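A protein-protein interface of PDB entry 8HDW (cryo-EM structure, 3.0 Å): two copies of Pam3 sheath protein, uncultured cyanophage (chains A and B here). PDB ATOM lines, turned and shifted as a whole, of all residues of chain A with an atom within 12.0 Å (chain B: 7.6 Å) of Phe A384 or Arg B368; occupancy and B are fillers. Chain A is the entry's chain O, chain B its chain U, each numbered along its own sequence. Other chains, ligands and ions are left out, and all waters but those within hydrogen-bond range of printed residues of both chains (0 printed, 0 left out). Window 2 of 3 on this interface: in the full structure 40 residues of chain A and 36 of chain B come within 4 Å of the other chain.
Printed residues of chain A that touch a printed residue of chain B: Tyr A380, Thr A381, Met A382, Thr A383 and Phe A384.
Hydrophobic or aromatic side chains of chain A that line the printed part of chain B: Tyr A380 and Met A382.
Among the printed residues, 12 pairs touch across the chains.
The backbone carbonyl oxygen (O) of Thr A381 sits at hydrogen-bond distance from the backbone NH (N) of Phe B367 (3.2 Å).
OG1 of Thr A381 lies within hydrogen-bond range of NE of Arg B366 (3.0 Å).
The side-chain sulfur of Met B316 sits close to the side-chain hydroxyl of Tyr A380, at 3.8 Å.
Of chain A, only Thr A383 and Phe A384 come within 4 Å of Arg B368.
No residue of chain A comes within 4 Å of Val B325.
No residue of chain A comes within 4 Å of Ala B326.
No residue of chain A comes within 4 Å of Asn B330.
No residue of chain A comes within 4 Å of Glu B337.
No residue of chain A comes within 4 Å of Ala B339.
Of chain A, only Thr A381, Met A382 and Thr A383 come within 4 Å of Arg B366.
Of the printed residues of chain A, Phe B367 touches Tyr A380 (3.7 Å), Thr A381 (3.2 Å), Met A382 (3.3 Å) and Thr A383 (3.0 Å).
Of chain A, only Met A382 and Phe A384 come within 4 Å of Tyr B369.
No residue of chain A comes within 4 Å of Gly B371.
Of the printed residues of chain B, Tyr A380 touches Met B316 (3.6 Å) and Phe B367 (3.7 Å).
Of the printed residues of chain B, Thr A381 touches Arg B366 (3.0 Å) and Phe B367 (3.2 Å).
Leu B332 touches none of the printed residues of chain A.
The nearest residue of chain A that does not touch Arg B368 is Met A382 (5.1 Å).
Tyr A380 touches Phe B367.
Met A382 touches Arg B366.
Met A382 touches Phe B367.
SD of Met A382 touches CD2 of Tyr B369, 3.3 Å away.
Thr A383 touches Arg B366 (CG2 to CZ, 3.3 Å).
CG2 of Thr A383 touches O of Phe B367, at 3.0 Å.
OG1 of Thr A383 touches NH2 of Arg B368 (3.5 Å).
C of Phe A384 touches NE of Arg B368 (3.8 Å).
Phe A384 touches Tyr B369 (CA to N, 3.5 Å).
No position is printed for both chains.
Of the 12 pairs that touch across the chains among the printed residues, none has its exchanged pair printed and touching as well.
The side-chain carboxylate (OE1) of Glu B337 lies within salt-bridge range of the guanidinium group (NH1) of Arg B368 (2.4 Å).
The backbone NH (N) of Ala B326 lies within hydrogen-bond range of the backbone carbonyl oxygen (O) of Arg B368, 3.1 Å away.
The backbone carbonyl oxygen (O) of Glu B273 lies within hydrogen-bond range of the side-chain hydroxyl (OH) of Tyr B369.
The backbone carbonyl oxygen (O) of Thr B341 sits at hydrogen-bond distance from the backbone NH (N) of Arg B366 (3.0 Å).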
ATOM      1  N   ASN A 379     -13.894  22.979  -1.290  1.00  0.00           N
ATOM      2  CA  ASN A 379     -15.295  22.594  -1.113  1.00  0.00           C
ATOM      3  C   ASN A 379     -15.628  21.147  -1.459  1.00  0.00           C
ATOM      4  O   ASN A 379     -16.304  20.492  -0.665  1.00  0.00           O
ATOM      5  CB  ASN A 379     -16.198  23.529  -1.913  1.00  0.00           C
ATOM      6  CG  ASN A 379     -16.374  24.868  -1.237  1.00  0.00           C
ATOM      7  OD1 ASN A 379     -16.097  25.011  -0.050  1.00  0.00           O
ATOM      8  ND2 ASN A 379     -16.838  25.855  -1.988  1.00  0.00           N
ATOM      9  N   TYR A 380     -15.210  20.621  -2.614  1.00  0.00           N
ATOM     10  CA  TYR A 380     -15.314  19.185  -2.915  1.00  0.00           C
ATOM     11  C   TYR A 380     -16.762  18.678  -2.908  1.00  0.00           C
ATOM     12  O   TYR A 380     -17.174  17.929  -2.026  1.00  0.00           O
ATOM     13  CB  TYR A 380     -14.486  18.358  -1.928  1.00  0.00           C
ATOM     14  CG  TYR A 380     -13.073  18.073  -2.352  1.00  0.00           C
ATOM     15  CD1 TYR A 380     -12.791  17.605  -3.618  1.00  0.00           C
ATOM     16  CD2 TYR A 380     -12.019  18.271  -1.476  1.00  0.00           C
ATOM     17  CE1 TYR A 380     -11.504  17.348  -4.001  1.00  0.00           C
ATOM     18  CE2 TYR A 380     -10.733  18.018  -1.854  1.00  0.00           C
ATOM     19  CZ  TYR A 380     -10.482  17.557  -3.117  1.00  0.00           C
ATOM     20  OH  TYR A 380      -9.193  17.299  -3.502  1.00  0.00           O
ATOM     21  N   THR A 381     -17.538  19.101  -3.903  1.00  0.00           N
ATOM     22  CA  THR A 381     -18.860  18.516  -4.133  1.00  0.00           C
ATOM     23  C   THR A 381     -18.718  17.169  -4.837  1.00  0.00           C
ATOM     24  O   THR A 381     -17.865  17.007  -5.712  1.00  0.00           O
ATOM     25  CB  THR A 381     -19.752  19.443  -4.955  1.00  0.00           C
ATOM     26  OG1 THR A 381     -19.050  19.882  -6.121  1.00  0.00           O
ATOM     27  CG2 THR A 381     -20.166  20.645  -4.136  1.00  0.00           C
ATOM     28  N   MET A 382     -19.557  16.210  -4.458  1.00  0.00           N
ATOM     29  CA  MET A 382     -19.511  14.853  -4.987  1.00  0.00           C
ATOM     30  C   MET A 382     -20.843  14.512  -5.640  1.00  0.00           C
ATOM     31  O   MET A 382     -21.901  14.846  -5.099  1.00  0.00           O
ATOM     32  CB  MET A 382     -19.192  13.856  -3.875  1.00  0.00           C
ATOM     33  CG  MET A 382     -18.768  12.494  -4.356  1.00  0.00           C
ATOM     34  SD  MET A 382     -18.401  11.394  -2.981  1.00  0.00           S
ATOM     35  CE  MET A 382     -19.999  11.317  -2.193  1.00  0.00           C
ATOM     36  N   THR A 383     -20.797  13.857  -6.799  1.00  0.00           N
ATOM     37  CA  THR A 383     -22.016  13.633  -7.572  1.00  0.00           C
ATOM     38  C   THR A 383     -22.318  12.173  -7.866  1.00  0.00           C
ATOM     39  O   THR A 383     -23.462  11.858  -8.202  1.00  0.00           O
ATOM     40  CB  THR A 383     -21.967  14.385  -8.906  1.00  0.00           C
ATOM     41  OG1 THR A 383     -22.419  13.518  -9.951  1.00  0.00           O
ATOM     42  CG2 THR A 383     -20.563  14.844  -9.214  1.00  0.00           C
ATOM     43  N   PHE A 384     -21.335  11.285  -7.773  1.00  0.00           N
ATOM     44  CA  PHE A 384     -21.548   9.868  -8.057  1.00  0.00           C
ATOM     45  C   PHE A 384     -22.066   9.649  -9.471  1.00  0.00           C
ATOM     46  O   PHE A 384     -21.851   8.591 -10.068  1.00  0.00           O
ATOM     47  CB  PHE A 384     -22.519   9.250  -7.040  1.00  0.00           C
ATOM     48  CG  PHE A 384     -23.090   7.931  -7.469  1.00  0.00           C
ATOM     49  CD1 PHE A 384     -22.368   6.764  -7.309  1.00  0.00           C
ATOM     50  CD2 PHE A 384     -24.356   7.857  -8.027  1.00  0.00           C
ATOM     51  CE1 PHE A 384     -22.892   5.545  -7.706  1.00  0.00           C
ATOM     52  CE2 PHE A 384     -24.887   6.645  -8.422  1.00  0.00           C
ATOM     53  CZ  PHE A 384     -24.154   5.488  -8.261  1.00  0.00           C
ATOM     54  N   GLU B 273     -17.193   4.072   0.973  1.00  0.00           N
ATOM     55  CA  GLU B 273     -17.350   5.427   0.464  1.00  0.00           C
ATOM     56  C   GLU B 273     -16.878   6.451   1.483  1.00  0.00           C
ATOM     57  O   GLU B 273     -16.073   7.335   1.158  1.00  0.00           O
ATOM     58  CB  GLU B 273     -18.805   5.701   0.099  1.00  0.00           C
ATOM     59  CG  GLU B 273     -19.456   4.639  -0.742  1.00  0.00           C
ATOM     60  CD  GLU B 273     -20.958   4.803  -0.792  1.00  0.00           C
ATOM     61  OE1 GLU B 273     -21.449   5.870  -0.371  1.00  0.00           O
ATOM     62  OE2 GLU B 273     -21.651   3.866  -1.240  1.00  0.00           O
ATOM     63  N   MET B 316      -6.465  14.593  -6.857  1.00  0.00           N
ATOM     64  CA  MET B 316      -7.473  13.949  -7.694  1.00  0.00           C
ATOM     65  C   MET B 316      -6.844  12.944  -8.651  1.00  0.00           C
ATOM     66  O   MET B 316      -7.432  11.896  -8.933  1.00  0.00           O
ATOM     67  CB  MET B 316      -8.281  14.993  -8.460  1.00  0.00           C
ATOM     68  CG  MET B 316      -9.130  15.888  -7.586  1.00  0.00           C
ATOM     69  SD  MET B 316     -10.097  15.015  -6.341  1.00  0.00           S
ATOM     70  CE  MET B 316     -11.253  14.139  -7.365  1.00  0.00           C
ATOM     71  N   GLY B 323      -8.797   4.054  -7.923  1.00  0.00           N
ATOM     72  CA  GLY B 323     -10.051   3.492  -8.372  1.00  0.00           C
ATOM     73  C   GLY B 323     -11.251   4.088  -7.673  1.00  0.00           C
ATOM     74  O   GLY B 323     -12.358   3.558  -7.777  1.00  0.00           O
ATOM     75  N   ILE B 324     -11.045   5.193  -6.962  1.00  0.00           N
ATOM     76  CA  ILE B 324     -12.107   5.836  -6.198  1.00  0.00           C
ATOM     77  C   ILE B 324     -12.893   6.770  -7.108  1.00  0.00           C
ATOM     78  O   ILE B 324     -14.120   6.857  -7.013  1.00  0.00           O
ATOM     79  CB  ILE B 324     -11.531   6.590  -4.987  1.00  0.00           C
ATOM     80  CG1 ILE B 324     -10.799   5.626  -4.059  1.00  0.00           C
ATOM     81  CG2 ILE B 324     -12.622   7.315  -4.230  1.00  0.00           C
ATOM     82  CD1 ILE B 324      -9.995   6.318  -2.997  1.00  0.00           C
ATOM     83  N   VAL B 325     -12.197   7.459  -8.004  1.00  0.00           N
ATOM     84  CA  VAL B 325     -12.814   8.385  -8.944  1.00  0.00           C
ATOM     85  C   VAL B 325     -13.061   7.649 -10.254  1.00  0.00           C
ATOM     86  O   VAL B 325     -12.307   6.748 -10.636  1.00  0.00           O
ATOM     87  CB  VAL B 325     -11.934   9.639  -9.140  1.00  0.00           C
ATOM     88  CG1 VAL B 325     -12.558  10.602 -10.118  1.00  0.00           C
ATOM     89  CG2 VAL B 325     -11.723  10.331  -7.814  1.00  0.00           C
ATOM     90  N   ALA B 326     -14.139   8.028 -10.938  1.00  0.00           N
ATOM     91  CA  ALA B 326     -14.621   7.291 -12.093  1.00  0.00           C
ATOM     92  C   ALA B 326     -13.744   7.524 -13.322  1.00  0.00           C
ATOM     93  O   ALA B 326     -12.833   8.354 -13.330  1.00  0.00           O
ATOM     94  CB  ALA B 326     -16.060   7.680 -12.408  1.00  0.00           C
ATOM     95  N   LEU B 327     -14.034   6.759 -14.371  1.00  0.00           N
ATOM     96  CA  LEU B 327     -13.243   6.754 -15.602  1.00  0.00           C
ATOM     97  C   LEU B 327     -13.913   7.564 -16.714  1.00  0.00           C
ATOM     98  O   LEU B 327     -14.300   7.029 -17.749  1.00  0.00           O
ATOM     99  CB  LEU B 327     -12.991   5.319 -16.054  1.00  0.00           C
ATOM    100  CG  LEU B 327     -11.948   5.094 -17.149  1.00  0.00           C
ATOM    101  CD1 LEU B 327     -10.545   5.076 -16.564  1.00  0.00           C
ATOM    102  CD2 LEU B 327     -12.240   3.819 -17.918  1.00  0.00           C
ATOM    103  N   ASP B 328     -14.069   8.864 -16.483  1.00  0.00           N
ATOM    104  CA  ASP B 328     -14.169   9.864 -17.556  1.00  0.00           C
ATOM    105  C   ASP B 328     -15.251   9.562 -18.596  1.00  0.00           C
ATOM    106  O   ASP B 328     -15.197  10.047 -19.724  1.00  0.00           O
ATOM    107  CB  ASP B 328     -12.818  10.017 -18.249  1.00  0.00           C
ATOM    108  CG  ASP B 328     -12.399  11.457 -18.403  1.00  0.00           C
ATOM    109  OD1 ASP B 328     -13.057  12.333 -17.814  1.00  0.00           O
ATOM    110  OD2 ASP B 328     -11.404  11.713 -19.108  1.00  0.00           O
ATOM    111  N   LEU B 329     -16.250   8.764 -18.229  1.00  0.00           N
ATOM    112  CA  LEU B 329     -17.315   8.408 -19.164  1.00  0.00           C
ATOM    113  C   LEU B 329     -18.657   8.537 -18.468  1.00  0.00           C
ATOM    114  O   LEU B 329     -18.777   8.206 -17.287  1.00  0.00           O
ATOM    115  CB  LEU B 329     -17.132   6.991 -19.711  1.00  0.00           C
ATOM    116  CG  LEU B 329     -15.985   6.783 -20.698  1.00  0.00           C
ATOM    117  CD1 LEU B 329     -15.797   5.318 -20.991  1.00  0.00           C
ATOM    118  CD2 LEU B 329     -16.229   7.550 -21.977  1.00  0.00           C
ATOM    119  N   ASN B 330     -19.654   9.006 -19.197  1.00  0.00           N
ATOM    120  CA  ASN B 330     -20.995   9.174 -18.649  1.00  0.00           C
ATOM    121  C   ASN B 330     -21.580   7.819 -18.276  1.00  0.00           C
ATOM    122  O   ASN B 330     -21.658   6.933 -19.135  1.00  0.00           O
ATOM    123  CB  ASN B 330     -21.879   9.875 -19.675  1.00  0.00           C
ATOM    124  CG  ASN B 330     -23.151  10.416 -19.079  1.00  0.00           C
ATOM    125  OD1 ASN B 330     -23.202  10.767 -17.906  1.00  0.00           O
ATOM    126  ND2 ASN B 330     -24.192  10.492 -19.890  1.00  0.00           N
ATOM    127  N   PRO B 331     -21.994   7.603 -17.025  1.00  0.00           N
ATOM    128  CA  PRO B 331     -22.535   6.287 -16.654  1.00  0.00           C
ATOM    129  C   PRO B 331     -23.863   5.971 -17.314  1.00  0.00           C
ATOM    130  O   PRO B 331     -24.233   4.797 -17.407  1.00  0.00           O
ATOM    131  CB  PRO B 331     -22.674   6.385 -15.131  1.00  0.00           C
ATOM    132  CG  PRO B 331     -21.859   7.559 -14.732  1.00  0.00           C
ATOM    133  CD  PRO B 331     -21.929   8.508 -15.872  1.00  0.00           C
ATOM    134  N   LEU B 332     -24.602   6.987 -17.761  1.00  0.00           N
ATOM    135  CA  LEU B 332     -25.895   6.751 -18.390  1.00  0.00           C
ATOM    136  C   LEU B 332     -25.725   6.250 -19.819  1.00  0.00           C
ATOM    137  O   LEU B 332     -26.252   5.196 -20.185  1.00  0.00           O
ATOM    138  CB  LEU B 332     -26.720   8.039 -18.363  1.00  0.00           C
ATOM    139  CG  LEU B 332     -28.256   8.061 -18.360  1.00  0.00           C
ATOM    140  CD1 LEU B 332     -28.879   6.892 -19.110  1.00  0.00           C
ATOM    141  CD2 LEU B 332     -28.807   8.155 -16.953  1.00  0.00           C
ATOM    142  N   ALA B 335     -21.071   8.259 -23.131  1.00  0.00           N
ATOM    143  CA  ALA B 335     -20.444   9.365 -23.828  1.00  0.00           C
ATOM    144  C   ALA B 335     -19.393  10.014 -22.934  1.00  0.00           C
ATOM    145  O   ALA B 335     -19.353   9.799 -21.723  1.00  0.00           O
ATOM    146  CB  ALA B 335     -21.499  10.373 -24.268  1.00  0.00           C
ATOM    147  N   GLU B 337     -17.445  12.449 -20.594  1.00  0.00           N
ATOM    148  CA  GLU B 337     -17.751  13.444 -19.578  1.00  0.00           C
ATOM    149  C   GLU B 337     -16.575  13.556 -18.618  1.00  0.00           C
ATOM    150  O   GLU B 337     -16.028  12.532 -18.198  1.00  0.00           O
ATOM    151  CB  GLU B 337     -19.027  13.071 -18.829  1.00  0.00           C
ATOM    152  CG  GLU B 337     -19.673  14.225 -18.114  1.00  0.00           C
ATOM    153  CD  GLU B 337     -20.855  13.795 -17.287  1.00  0.00           C
ATOM    154  OE1 GLU B 337     -21.028  12.574 -17.101  1.00  0.00           O
ATOM    155  OE2 GLU B 337     -21.612  14.672 -16.823  1.00  0.00           O
ATOM    156  N   PRO B 338     -16.145  14.767 -18.262  1.00  0.00           N
ATOM    157  CA  PRO B 338     -15.020  14.906 -17.328  1.00  0.00           C
ATOM    158  C   PRO B 338     -15.330  14.282 -15.975  1.00  0.00           C
ATOM    159  O   PRO B 338     -16.436  14.411 -15.451  1.00  0.00           O
ATOM    160  CB  PRO B 338     -14.840  16.422 -17.213  1.00  0.00           C
ATOM    161  CG  PRO B 338     -15.524  16.987 -18.385  1.00  0.00           C
ATOM    162  CD  PRO B 338     -16.642  16.070 -18.722  1.00  0.00           C
ATOM    163  N   ALA B 339     -14.331  13.608 -15.405  1.00  0.00           N
ATOM    164  CA  ALA B 339     -14.528  12.948 -14.117  1.00  0.00           C
ATOM    165  C   ALA B 339     -14.497  13.949 -12.969  1.00  0.00           C
ATOM    166  O   ALA B 339     -15.285  13.844 -12.025  1.00  0.00           O
ATOM    167  CB  ALA B 339     -13.476  11.861 -13.915  1.00  0.00           C
ATOM    168  N   TYR B 340     -13.596  14.928 -13.032  1.00  0.00           N
ATOM    169  CA  TYR B 340     -13.471  15.934 -11.990  1.00  0.00           C
ATOM    170  C   TYR B 340     -13.030  17.258 -12.593  1.00  0.00           C
ATOM    171  O   TYR B 340     -12.295  17.279 -13.580  1.00  0.00           O
ATOM    172  CB  TYR B 340     -12.476  15.496 -10.910  1.00  0.00           C
ATOM    173  CG  TYR B 340     -11.107  15.108 -11.412  1.00  0.00           C
ATOM    174  CD1 TYR B 340     -10.809  13.792 -11.718  1.00  0.00           C
ATOM    175  CD2 TYR B 340     -10.105  16.055 -11.555  1.00  0.00           C
ATOM    176  CE1 TYR B 340      -9.565  13.433 -12.166  1.00  0.00           C
ATOM    177  CE2 TYR B 340      -8.856  15.704 -12.004  1.00  0.00           C
ATOM    178  CZ  TYR B 340      -8.590  14.391 -12.307  1.00  0.00           C
ATOM    179  OH  TYR B 340      -7.343  14.028 -12.753  1.00  0.00           O
ATOM    180  N   THR B 341     -13.481  18.359 -11.994  1.00  0.00           N
ATOM    181  CA  THR B 341     -13.044  19.697 -12.370  1.00  0.00           C
ATOM    182  C   THR B 341     -12.619  20.459 -11.126  1.00  0.00           C
ATOM    183  O   THR B 341     -13.093  20.175 -10.026  1.00  0.00           O
ATOM    184  CB  THR B 341     -14.138  20.493 -13.088  1.00  0.00           C
ATOM    185  OG1 THR B 341     -15.116  20.924 -12.137  1.00  0.00           O
ATOM    186  CG2 THR B 341     -14.814  19.651 -14.162  1.00  0.00           C
ATOM    187  N   ARG B 366     -14.942  19.044  -8.023  1.00  0.00           N
ATOM    188  CA  ARG B 366     -16.049  18.212  -8.474  1.00  0.00           C
ATOM    189  C   ARG B 366     -15.625  16.753  -8.531  1.00  0.00           C
ATOM    190  O   ARG B 366     -14.447  16.444  -8.721  1.00  0.00           O
ATOM    191  CB  ARG B 366     -16.540  18.644  -9.844  1.00  0.00           C
ATOM    192  CG  ARG B 366     -17.562  19.743  -9.825  1.00  0.00           C
ATOM    193  CD  ARG B 366     -18.940  19.179 -10.020  1.00  0.00           C
ATOM    194  NE  ARG B 366     -19.495  18.645  -8.783  1.00  0.00           N
ATOM    195  CZ  ARG B 366     -20.719  18.137  -8.676  1.00  0.00           C
ATOM    196  NH1 ARG B 366     -21.512  18.090  -9.738  1.00  0.00           N
ATOM    197  NH2 ARG B 366     -21.149  17.674  -7.514  1.00  0.00           N
ATOM    198  N   PHE B 367     -16.593  15.863  -8.388  1.00  0.00           N
ATOM    199  CA  PHE B 367     -16.343  14.456  -8.141  1.00  0.00           C
ATOM    200  C   PHE B 367     -17.070  13.576  -9.147  1.00  0.00           C
ATOM    201  O   PHE B 367     -17.805  14.042 -10.014  1.00  0.00           O
ATOM    202  CB  PHE B 367     -16.814  14.095  -6.741  1.00  0.00           C
ATOM    203  CG  PHE B 367     -15.730  13.668  -5.806  1.00  0.00           C
ATOM    204  CD1 PHE B 367     -15.058  14.599  -5.045  1.00  0.00           C
ATOM    205  CD2 PHE B 367     -15.434  12.330  -5.644  1.00  0.00           C
ATOM    206  CE1 PHE B 367     -14.097  14.211  -4.168  1.00  0.00           C
ATOM    207  CE2 PHE B 367     -14.475  11.937  -4.770  1.00  0.00           C
ATOM    208  CZ  PHE B 367     -13.802  12.878  -4.026  1.00  0.00           C
ATOM    209  N   ARG B 368     -16.823  12.275  -9.032  1.00  0.00           N
ATOM    210  CA  ARG B 368     -17.740  11.245  -9.509  1.00  0.00           C
ATOM    211  C   ARG B 368     -17.239   9.942  -8.910  1.00  0.00           C
ATOM    212  O   ARG B 368     -16.059   9.615  -9.052  1.00  0.00           O
ATOM    213  CB  ARG B 368     -17.796  11.181 -11.026  1.00  0.00           C
ATOM    214  CG  ARG B 368     -18.692  10.076 -11.550  1.00  0.00           C
ATOM    215  CD  ARG B 368     -19.360  10.463 -12.851  1.00  0.00           C
ATOM    216  NE  ARG B 368     -20.637  11.130 -12.619  1.00  0.00           N
ATOM    217  CZ  ARG B 368     -21.334  11.765 -13.556  1.00  0.00           C
ATOM    218  NH1 ARG B 368     -20.877  11.830 -14.797  1.00  0.00           N
ATOM    219  NH2 ARG B 368     -22.489  12.342 -13.251  1.00  0.00           N
ATOM    220  N   TYR B 369     -18.120   9.220  -8.229  1.00  0.00           N
ATOM    221  CA  TYR B 369     -17.702   8.022  -7.523  1.00  0.00           C
ATOM    222  C   TYR B 369     -17.758   6.805  -8.434  1.00  0.00           C
ATOM    223  O   TYR B 369     -18.603   6.711  -9.326  1.00  0.00           O
ATOM    224  CB  TYR B 369     -18.585   7.801  -6.300  1.00  0.00           C
ATOM    225  CG  TYR B 369     -17.794   7.485  -5.070  1.00  0.00           C
ATOM    226  CD1 TYR B 369     -16.884   6.444  -5.059  1.00  0.00           C
ATOM    227  CD2 TYR B 369     -17.930   8.247  -3.929  1.00  0.00           C
ATOM    228  CE1 TYR B 369     -16.142   6.158  -3.941  1.00  0.00           C
ATOM    229  CE2 TYR B 369     -17.190   7.972  -2.801  1.00  0.00           C
ATOM    230  CZ  TYR B 369     -16.298   6.926  -2.816  1.00  0.00           C
ATOM    231  OH  TYR B 369     -15.552   6.646  -1.700  1.00  0.00           O
ATOM    232  N   ALA B 370     -16.845   5.870  -8.205  1.00  0.00           N
ATOM    233  CA  ALA B 370     -16.830   4.595  -8.905  1.00  0.00           C
ATOM    234  C   ALA B 370     -17.145   3.487  -7.908  1.00  0.00           C
ATOM    235  O   ALA B 370     -16.331   3.194  -7.026  1.00  0.00           O
ATOM    236  CB  ALA B 370     -15.479   4.360  -9.576  1.00  0.00           C
ATOM    237  N   GLY B 371     -18.318   2.879  -8.048  1.00  0.00           N
ATOM    238  CA  GLY B 371     -18.755   1.840  -7.140  1.00  0.00           C
ATOM    239  C   GLY B 371     -18.265   0.464  -7.561  1.00  0.00           C
ATOM    240  O   GLY B 371     -17.391   0.299  -8.412  1.00  0.00           O
ATOM    241  N   ALA B 372     -18.855  -0.550  -6.935  1.00  0.00           N
ATOM    242  CA  ALA B 372     -18.501  -1.929  -7.233  1.00  0.00           C
ATOM    243  C   ALA B 372     -19.755  -2.792  -7.119  1.00  0.00           C
ATOM    244  O   ALA B 372     -20.865  -2.282  -6.957  1.00  0.00           O
ATOM    245  CB  ALA B 372     -17.358  -2.385  -6.323  1.00  0.00           C
